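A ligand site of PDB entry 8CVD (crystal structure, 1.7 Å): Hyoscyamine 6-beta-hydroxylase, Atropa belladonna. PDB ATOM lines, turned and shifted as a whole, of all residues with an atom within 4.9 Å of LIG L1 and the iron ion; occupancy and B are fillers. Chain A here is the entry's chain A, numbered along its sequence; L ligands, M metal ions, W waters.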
ATOM      1  N   PHE A 103      26.358 -23.180   3.759  1.00  0.00           N
ATOM      2  CA  PHE A 103      25.754 -22.643   2.519  1.00  0.00           C
ATOM      3  C   PHE A 103      24.599 -21.724   2.918  1.00  0.00           C
ATOM      4  O   PHE A 103      23.456 -22.176   3.063  1.00  0.00           O
ATOM      5  CB  PHE A 103      25.358 -23.789   1.576  1.00  0.00           C
ATOM      6  CG  PHE A 103      26.526 -24.453   0.909  1.00  0.00           C
ATOM      7  CD1 PHE A 103      27.259 -23.793  -0.067  1.00  0.00           C
ATOM      8  CD2 PHE A 103      26.914 -25.746   1.263  1.00  0.00           C
ATOM      9  CE1 PHE A 103      28.340 -24.412  -0.687  1.00  0.00           C
ATOM     10  CE2 PHE A 103      27.989 -26.353   0.631  1.00  0.00           C
ATOM     11  CZ  PHE A 103      28.700 -25.691  -0.339  1.00  0.00           C
ATOM     12  N   LEU A 105      23.776 -17.030   2.819  1.00  0.00           N
ATOM     13  CA  LEU A 105      24.237 -15.702   2.353  1.00  0.00           C
ATOM     14  C   LEU A 105      24.720 -14.912   3.566  1.00  0.00           C
ATOM     15  O   LEU A 105      24.158 -15.065   4.655  1.00  0.00           O
ATOM     16  CB  LEU A 105      23.084 -15.004   1.621  1.00  0.00           C
ATOM     17  CG  LEU A 105      22.463 -15.806   0.479  1.00  0.00           C
ATOM     18  CD1 LEU A 105      21.430 -14.988  -0.270  1.00  0.00           C
ATOM     19  CD2 LEU A 105      23.533 -16.323  -0.475  1.00  0.00           C
ATOM     20  N   LEU A 107      27.393 -15.679   0.674  1.00  0.00           N
ATOM     21  CA  LEU A 107      28.239 -16.802   0.204  1.00  0.00           C
ATOM     22  C   LEU A 107      29.514 -16.202  -0.394  1.00  0.00           C
ATOM     23  O   LEU A 107      29.489 -15.751  -1.557  1.00  0.00           O
ATOM     24  CB  LEU A 107      27.462 -17.651  -0.811  1.00  0.00           C
ATOM     25  CG  LEU A 107      28.086 -19.007  -1.139  1.00  0.00           C
ATOM     26  CD1 LEU A 107      28.177 -19.885   0.101  1.00  0.00           C
ATOM     27  CD2 LEU A 107      27.301 -19.726  -2.238  1.00  0.00           C
ATOM     28  N   GLU A 116      26.824 -29.340   4.840  1.00  0.00           N
ATOM     29  CA  GLU A 116      25.512 -29.109   4.206  1.00  0.00           C
ATOM     30  C   GLU A 116      24.512 -30.153   4.709  1.00  0.00           C
ATOM     31  O   GLU A 116      24.936 -31.276   5.040  1.00  0.00           O
ATOM     32  CB  GLU A 116      25.636 -29.155   2.681  1.00  0.00           C
ATOM     33  CG  GLU A 116      24.420 -28.604   1.966  1.00  0.00           C
ATOM     34  CD  GLU A 116      24.531 -28.569   0.455  1.00  0.00           C
ATOM     35  OE1 GLU A 116      25.538 -29.076  -0.092  1.00  0.00           O
ATOM     36  OE2 GLU A 116      23.610 -28.004  -0.185  1.00  0.00           O
ATOM     37  N   TYR A 127      24.285 -33.996   5.164  1.00  0.00           N
ATOM     38  CA  TYR A 127      24.750 -34.733   3.973  1.00  0.00           C
ATOM     39  C   TYR A 127      26.108 -35.374   4.292  1.00  0.00           C
ATOM     40  O   TYR A 127      26.936 -34.720   4.945  1.00  0.00           O
ATOM     41  CB  TYR A 127      24.854 -33.816   2.757  1.00  0.00           C
ATOM     42  CG  TYR A 127      23.551 -33.218   2.293  1.00  0.00           C
ATOM     43  CD1 TYR A 127      22.323 -33.761   2.648  1.00  0.00           C
ATOM     44  CD2 TYR A 127      23.546 -32.094   1.478  1.00  0.00           C
ATOM     45  CE1 TYR A 127      21.129 -33.199   2.236  1.00  0.00           C
ATOM     46  CE2 TYR A 127      22.358 -31.529   1.036  1.00  0.00           C
ATOM     47  CZ  TYR A 127      21.143 -32.077   1.425  1.00  0.00           C
ATOM     48  OH  TYR A 127      19.989 -31.515   0.970  1.00  0.00           O
ATOM     49  N   LYS A 129      29.133 -35.693   3.197  1.00  0.00           N
ATOM     50  CA  LYS A 129      29.860 -34.898   2.177  1.00  0.00           C
ATOM     51  C   LYS A 129      30.707 -33.827   2.884  1.00  0.00           C
ATOM     52  O   LYS A 129      30.188 -33.184   3.831  1.00  0.00           O
ATOM     53  CB  LYS A 129      28.860 -34.246   1.229  1.00  0.00           C
ATOM     54  CG  LYS A 129      29.421 -33.216   0.251  1.00  0.00           C
ATOM     55  CD  LYS A 129      28.414 -32.786  -0.796  1.00  0.00           C
ATOM     56  CE  LYS A 129      27.358 -31.849  -0.261  1.00  0.00           C
ATOM     57  NZ  LYS A 129      27.887 -30.481  -0.033  1.00  0.00           N
ATOM     58  N   MET A 196      31.146 -20.504  -8.878  1.00  0.00           N
ATOM     59  CA  MET A 196      31.524 -21.220  -7.637  1.00  0.00           C
ATOM     60  C   MET A 196      32.007 -22.614  -8.050  1.00  0.00           C
ATOM     61  O   MET A 196      31.228 -23.345  -8.687  1.00  0.00           O
ATOM     62  CB  MET A 196      30.344 -21.339  -6.668  1.00  0.00           C
ATOM     63  CG  MET A 196      29.874 -20.000  -6.103  1.00  0.00           C
ATOM     64  SD  MET A 196      31.189 -19.070  -5.255  1.00  0.00           S
ATOM     65  CE  MET A 196      31.601 -20.173  -3.910  1.00  0.00           C
ATOM     66  N   LEU A 198      32.757 -26.103  -6.591  1.00  0.00           N
ATOM     67  CA  LEU A 198      32.502 -26.990  -5.425  1.00  0.00           C
ATOM     68  C   LEU A 198      33.211 -28.309  -5.692  1.00  0.00           C
ATOM     69  O   LEU A 198      32.768 -29.029  -6.605  1.00  0.00           O
ATOM     70  CB  LEU A 198      31.004 -27.177  -5.247  1.00  0.00           C
ATOM     71  CG  LEU A 198      30.311 -26.079  -4.439  1.00  0.00           C
ATOM     72  CD1 LEU A 198      30.440 -24.738  -5.128  1.00  0.00           C
ATOM     73  CD2 LEU A 198      28.843 -26.426  -4.203  1.00  0.00           C
ATOM     74  N   SER A 214      24.061 -36.071  -1.094  1.00  0.00           N
ATOM     75  CA  SER A 214      23.236 -34.841  -1.166  1.00  0.00           C
ATOM     76  C   SER A 214      21.787 -35.243  -1.453  1.00  0.00           C
ATOM     77  O   SER A 214      21.570 -36.179  -2.241  1.00  0.00           O
ATOM     78  CB  SER A 214      23.752 -33.861  -2.198  1.00  0.00           C
ATOM     79  OG  SER A 214      23.725 -34.427  -3.493  1.00  0.00           O
ATOM     80  N   HIS A 217      17.732 -32.093  -5.376  1.00  0.00           N
ATOM     81  CA  HIS A 217      17.704 -30.614  -5.526  1.00  0.00           C
ATOM     82  C   HIS A 217      17.887 -30.228  -6.988  1.00  0.00           C
ATOM     83  O   HIS A 217      18.598 -30.950  -7.715  1.00  0.00           O
ATOM     84  CB  HIS A 217      18.780 -29.976  -4.637  1.00  0.00           C
ATOM     85  CG  HIS A 217      20.178 -30.281  -5.065  1.00  0.00           C
ATOM     86  ND1 HIS A 217      20.787 -31.489  -4.782  1.00  0.00           N
ATOM     87  CD2 HIS A 217      21.087 -29.563  -5.764  1.00  0.00           C
ATOM     88  CE1 HIS A 217      22.001 -31.496  -5.291  1.00  0.00           C
ATOM     89  NE2 HIS A 217      22.215 -30.322  -5.892  1.00  0.00           N
ATOM     90  N   ASP A 219      20.100 -27.360  -8.817  1.00  0.00           N
ATOM     91  CA  ASP A 219      21.107 -26.292  -8.590  1.00  0.00           C
ATOM     92  C   ASP A 219      20.348 -24.967  -8.774  1.00  0.00           C
ATOM     93  O   ASP A 219      19.599 -24.842  -9.756  1.00  0.00           O
ATOM     94  CB  ASP A 219      22.307 -26.442  -9.511  1.00  0.00           C
ATOM     95  CG  ASP A 219      23.262 -27.554  -9.106  1.00  0.00           C
ATOM     96  OD1 ASP A 219      22.993 -28.205  -8.081  1.00  0.00           O
ATOM     97  OD2 ASP A 219      24.240 -27.759  -9.833  1.00  0.00           O
ATOM     98  N   GLY A 220      20.494 -24.027  -7.837  1.00  0.00           N
ATOM     99  CA  GLY A 220      19.699 -22.785  -7.841  1.00  0.00           C
ATOM    100  C   GLY A 220      20.167 -21.790  -8.881  1.00  0.00           C
ATOM    101  O   GLY A 220      19.382 -20.900  -9.245  1.00  0.00           O
ATOM    102  N   ASN A 221      21.391 -21.969  -9.390  1.00  0.00           N
ATOM    103  CA  ASN A 221      22.102 -21.041 -10.301  1.00  0.00           C
ATOM    104  C   ASN A 221      21.616 -21.243 -11.752  1.00  0.00           C
ATOM    105  O   ASN A 221      20.545 -21.834 -11.940  1.00  0.00           O
ATOM    106  CB  ASN A 221      23.609 -21.219 -10.134  1.00  0.00           C
ATOM    107  CG  ASN A 221      24.027 -22.667 -10.215  1.00  0.00           C
ATOM    108  OD1 ASN A 221      23.705 -23.453  -9.313  1.00  0.00           O
ATOM    109  ND2 ASN A 221      24.706 -23.043 -11.285  1.00  0.00           N
ATOM    110  N   HIS A 273      18.686 -33.600  -9.088  1.00  0.00           N
ATOM    111  CA  HIS A 273      19.723 -34.651  -8.897  1.00  0.00           C
ATOM    112  C   HIS A 273      20.012 -34.835  -7.413  1.00  0.00           C
ATOM    113  O   HIS A 273      19.697 -33.938  -6.609  1.00  0.00           O
ATOM    114  CB  HIS A 273      20.979 -34.341  -9.724  1.00  0.00           C
ATOM    115  CG  HIS A 273      21.566 -33.003  -9.445  1.00  0.00           C
ATOM    116  ND1 HIS A 273      21.164 -31.861 -10.119  1.00  0.00           N
ATOM    117  CD2 HIS A 273      22.525 -32.604  -8.576  1.00  0.00           C
ATOM    118  CE1 HIS A 273      21.822 -30.819  -9.660  1.00  0.00           C
ATOM    119  NE2 HIS A 273      22.676 -31.244  -8.717  1.00  0.00           N
ATOM    120  N   LEU A 289      29.502 -24.157 -10.712  1.00  0.00           N
ATOM    121  CA  LEU A 289      28.151 -23.562 -10.643  1.00  0.00           C
ATOM    122  C   LEU A 289      28.257 -22.117 -11.115  1.00  0.00           C
ATOM    123  O   LEU A 289      28.846 -21.293 -10.400  1.00  0.00           O
ATOM    124  CB  LEU A 289      27.598 -23.646  -9.209  1.00  0.00           C
ATOM    125  CG  LEU A 289      27.108 -25.027  -8.784  1.00  0.00           C
ATOM    126  CD1 LEU A 289      28.261 -25.958  -8.488  1.00  0.00           C
ATOM    127  CD2 LEU A 289      26.203 -24.904  -7.565  1.00  0.00           C
ATOM    128  N   TYR A 294      24.324 -11.684  -6.793  1.00  0.00           N
ATOM    129  CA  TYR A 294      23.248 -11.607  -5.768  1.00  0.00           C
ATOM    130  C   TYR A 294      22.406 -10.341  -5.984  1.00  0.00           C
ATOM    131  O   TYR A 294      21.272 -10.310  -5.498  1.00  0.00           O
ATOM    132  CB  TYR A 294      23.858 -11.754  -4.376  1.00  0.00           C
ATOM    133  CG  TYR A 294      24.579 -13.070  -4.250  1.00  0.00           C
ATOM    134  CD1 TYR A 294      23.850 -14.257  -4.150  1.00  0.00           C
ATOM    135  CD2 TYR A 294      25.950 -13.158  -4.372  1.00  0.00           C
ATOM    136  CE1 TYR A 294      24.495 -15.487  -4.107  1.00  0.00           C
ATOM    137  CE2 TYR A 294      26.606 -14.379  -4.326  1.00  0.00           C
ATOM    138  CZ  TYR A 294      25.875 -15.547  -4.204  1.00  0.00           C
ATOM    139  OH  TYR A 294      26.516 -16.746  -4.170  1.00  0.00           O
ATOM    140  N   TYR A 318      17.556 -12.132  -6.840  1.00  0.00           N
ATOM    141  CA  TYR A 318      18.354 -13.382  -6.755  1.00  0.00           C
ATOM    142  C   TYR A 318      18.788 -13.617  -5.304  1.00  0.00           C
ATOM    143  O   TYR A 318      18.776 -14.775  -4.874  1.00  0.00           O
ATOM    144  CB  TYR A 318      19.545 -13.335  -7.716  1.00  0.00           C
ATOM    145  CG  TYR A 318      20.265 -14.654  -7.888  1.00  0.00           C
ATOM    146  CD1 TYR A 318      19.641 -15.737  -8.486  1.00  0.00           C
ATOM    147  CD2 TYR A 318      21.568 -14.804  -7.465  1.00  0.00           C
ATOM    148  CE1 TYR A 318      20.302 -16.940  -8.652  1.00  0.00           C
ATOM    149  CE2 TYR A 318      22.246 -16.010  -7.618  1.00  0.00           C
ATOM    150  CZ  TYR A 318      21.606 -17.081  -8.228  1.00  0.00           C
ATOM    151  OH  TYR A 318      22.294 -18.244  -8.407  1.00  0.00           O
ATOM    152  N   PHE A 321      15.684 -14.939  -3.385  1.00  0.00           N
ATOM    153  CA  PHE A 321      15.579 -16.336  -3.893  1.00  0.00           C
ATOM    154  C   PHE A 321      16.622 -17.203  -3.176  1.00  0.00           C
ATOM    155  O   PHE A 321      16.264 -18.292  -2.671  1.00  0.00           O
ATOM    156  CB  PHE A 321      15.761 -16.389  -5.406  1.00  0.00           C
ATOM    157  CG  PHE A 321      16.205 -17.741  -5.906  1.00  0.00           C
ATOM    158  CD1 PHE A 321      15.286 -18.762  -6.081  1.00  0.00           C
ATOM    159  CD2 PHE A 321      17.538 -18.007  -6.141  1.00  0.00           C
ATOM    160  CE1 PHE A 321      15.694 -20.017  -6.500  1.00  0.00           C
ATOM    161  CE2 PHE A 321      17.946 -19.262  -6.560  1.00  0.00           C
ATOM    162  CZ  PHE A 321      17.031 -20.262  -6.743  1.00  0.00           C
ATOM    163  N   GLY A 322      17.878 -16.756  -3.173  1.00  0.00           N
ATOM    164  CA  GLY A 322      19.033 -17.489  -2.617  1.00  0.00           C
ATOM    165  C   GLY A 322      18.801 -17.869  -1.166  1.00  0.00           C
ATOM    166  O   GLY A 322      19.048 -19.037  -0.803  1.00  0.00           O
ATOM    167  N   TYR A 325      16.137 -20.616  -1.167  1.00  0.00           N
ATOM    168  CA  TYR A 325      16.716 -21.815  -1.833  1.00  0.00           C
ATOM    169  C   TYR A 325      17.627 -22.571  -0.859  1.00  0.00           C
ATOM    170  O   TYR A 325      17.594 -23.822  -0.829  1.00  0.00           O
ATOM    171  CB  TYR A 325      17.460 -21.393  -3.100  1.00  0.00           C
ATOM    172  CG  TYR A 325      18.290 -22.504  -3.685  1.00  0.00           C
ATOM    173  CD1 TYR A 325      17.680 -23.587  -4.300  1.00  0.00           C
ATOM    174  CD2 TYR A 325      19.671 -22.491  -3.593  1.00  0.00           C
ATOM    175  CE1 TYR A 325      18.431 -24.636  -4.816  1.00  0.00           C
ATOM    176  CE2 TYR A 325      20.433 -23.531  -4.106  1.00  0.00           C
ATOM    177  CZ  TYR A 325      19.814 -24.603  -4.722  1.00  0.00           C
ATOM    178  OH  TYR A 325      20.577 -25.615  -5.223  1.00  0.00           O
ATOM    179  N   LEU A 326      18.438 -21.846  -0.082  1.00  0.00           N
ATOM    180  CA  LEU A 326      19.493 -22.455   0.779  1.00  0.00           C
ATOM    181  C   LEU A 326      18.904 -22.949   2.105  1.00  0.00           C
ATOM    182  O   LEU A 326      19.546 -23.827   2.715  1.00  0.00           O
ATOM    183  CB  LEU A 326      20.610 -21.428   0.997  1.00  0.00           C
ATOM    184  CG  LEU A 326      21.500 -21.175  -0.230  1.00  0.00           C
ATOM    185  CD1 LEU A 326      22.522 -20.072   0.045  1.00  0.00           C
ATOM    186  CD2 LEU A 326      22.191 -22.446  -0.682  1.00  0.00           C
HETATM  187  N1  LIG L   1      24.081 -28.219  -2.795  1.00  0.00           N
HETATM  188  C1  LIG L   1      23.706 -27.273  -4.912  1.00  0.00           C
HETATM  189  C2  LIG L   1      23.077 -27.452  -3.562  1.00  0.00           C
HETATM  190  C3  LIG L   1      25.421 -26.180  -2.521  1.00  0.00           C
HETATM  191  C4  LIG L   1      22.847 -26.119  -2.864  1.00  0.00           C
HETATM  192  C5  LIG L   1      24.036 -29.671  -2.976  1.00  0.00           C
HETATM  193  O1  LIG L   1      24.319 -24.517  -3.935  1.00  0.00           O
HETATM  194  O2  LIG L   1      26.214 -21.011  -6.444  1.00  0.00           O
HETATM  195  O3  LIG L   1      25.505 -23.016  -2.778  1.00  0.00           O
HETATM  196  C6  LIG L   1      23.839 -21.474  -5.018  1.00  0.00           C
HETATM  197  C7  LIG L   1      22.994 -21.290  -6.098  1.00  0.00           C
HETATM  198  C8  LIG L   1      21.993 -20.323  -6.062  1.00  0.00           C
HETATM  199  C9  LIG L   1      21.837 -19.531  -4.944  1.00  0.00           C
HETATM  200  C10 LIG L   1      22.676 -19.693  -3.873  1.00  0.00           C
HETATM  201  C11 LIG L   1      24.967 -23.344  -3.797  1.00  0.00           C
HETATM  202  C12 LIG L   1      25.146 -27.327  -4.699  1.00  0.00           C
HETATM  203  C13 LIG L   1      25.330 -27.531  -3.218  1.00  0.00           C
HETATM  204  C14 LIG L   1      24.158 -25.317  -2.723  1.00  0.00           C
HETATM  205  O4  LIG L   1      24.478 -28.385  -5.417  1.00  0.00           O
HETATM  206  C15 LIG L   1      24.947 -22.520  -5.067  1.00  0.00           C
HETATM  207  C16 LIG L   1      23.674 -20.661  -3.890  1.00  0.00           C
HETATM  208  C17 LIG L   1      26.310 -21.908  -5.338  1.00  0.00           C
HETATM  209  C1  LG2 L   2      27.921 -34.823  -7.623  1.00  0.00           C
HETATM  210  O1  LG2 L   2      27.985 -35.600  -8.585  1.00  0.00           O
HETATM  211  O2  LG2 L   2      28.706 -34.868  -6.668  1.00  0.00           O
HETATM  212  C2  LG2 L   2      26.796 -33.792  -7.598  1.00  0.00           C
HETATM  213  C3  LG2 L   2      27.145 -32.397  -7.130  1.00  0.00           C
HETATM  214  C4  LG2 L   2      25.961 -31.440  -7.113  1.00  0.00           C
HETATM  215  O3  LG2 L   2      24.939 -31.786  -6.495  1.00  0.00           O
HETATM  216  O4  LG2 L   2      26.056 -30.354  -7.736  1.00  0.00           O
HETATM  217 FE    FE M   1      23.714 -30.020  -7.354  1.00  0.00          FE
HETATM  218  O   HOH W   1      25.461 -30.378 -10.151  1.00  0.00           O
HETATM  219  O   HOH W   2      26.584 -19.830  -9.195  1.00  0.00           O
HETATM  220  O   HOH W   3      25.610 -18.475  -6.123  1.00  0.00           O
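A ring nitrogen (NE2) of His 217 sits close to an oxygen (O4) of LIG L1 (3.0 Å).
The side-chain carboxylate (OE2) of Glu 116 lies within salt-bridge range of a nitrogen (N1) of LIG L1 (2.7 Å).
The backbone carbonyl oxygen of Glu 116 lies within hydrogen-bond range of the backbone NH of Tyr 127 (2.8 Å).
The backbone carbonyl oxygen (O) of Met 196 lies within hydrogen-bond range of the backbone NH (N) of Leu 289 (2.8 Å).
The side-chain hydroxyl of Tyr 325 sits at hydrogen-bond distance from the backbone NH of Gly 220 (3.1 Å).
The side-chain carboxylate of Glu 116 lies within salt-bridge range of the side-chain amino group of Lys 129 (2.7 Å).
Phe 103 touches LIG L1 (CD1 to O3, 3.3 Å).
Leu 107 touches LIG L1.
Met 196 touches LIG L1.
Leu 198 touches LIG L1 (CD2 to C13, 3.8 Å).
Gly 220 touches LIG L1.
Asn 221 touches LIG L1.
Leu 289 touches LIG L1 (CD2 to C15, 3.7 Å).
Tyr 318 touches LIG L1.
OH of Tyr 325 touches C4 of LIG L1, at 3.3 Å.
Leu 326 touches LIG L1 (CD1 to C10, 3.9 Å).
13 residues have an atom within 4 Å of LIG L1: Phe 103, Leu 107, Glu 116, Met 196, Leu 198, His 217, Asp 219, Gly 220, Asn 221, Leu 289, Tyr 318, Tyr 325 and Leu 326.
Three residues have an atom within 4 Å of the iron ion: His 217, Asp 219 and His 273.
The iron ion is bound by the side-chain carboxylate (OD1) of Asp 219 (2.1 Å), a ring nitrogen (NE2) of His 273 (2.1 Å), a ring nitrogen (NE2) of His 217 (2.1 Å), an oxygen (O3) of LG2 L2 (2.3 Å) and an oxygen (O4) of LG2 L2 (2.4 Å).
The iron ion has five donor atoms within binding distance.
Slightly farther from the iron ion lies an oxygen (O4) of LIG L1 (2.6 Å).
Water W3 lies within hydrogen-bond range of O2 of LIG L1 and OH of Tyr 294.
Water W2 bridges O of Leu 289 (3.0 Å) and O2 of LIG L1 (3.0 Å).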
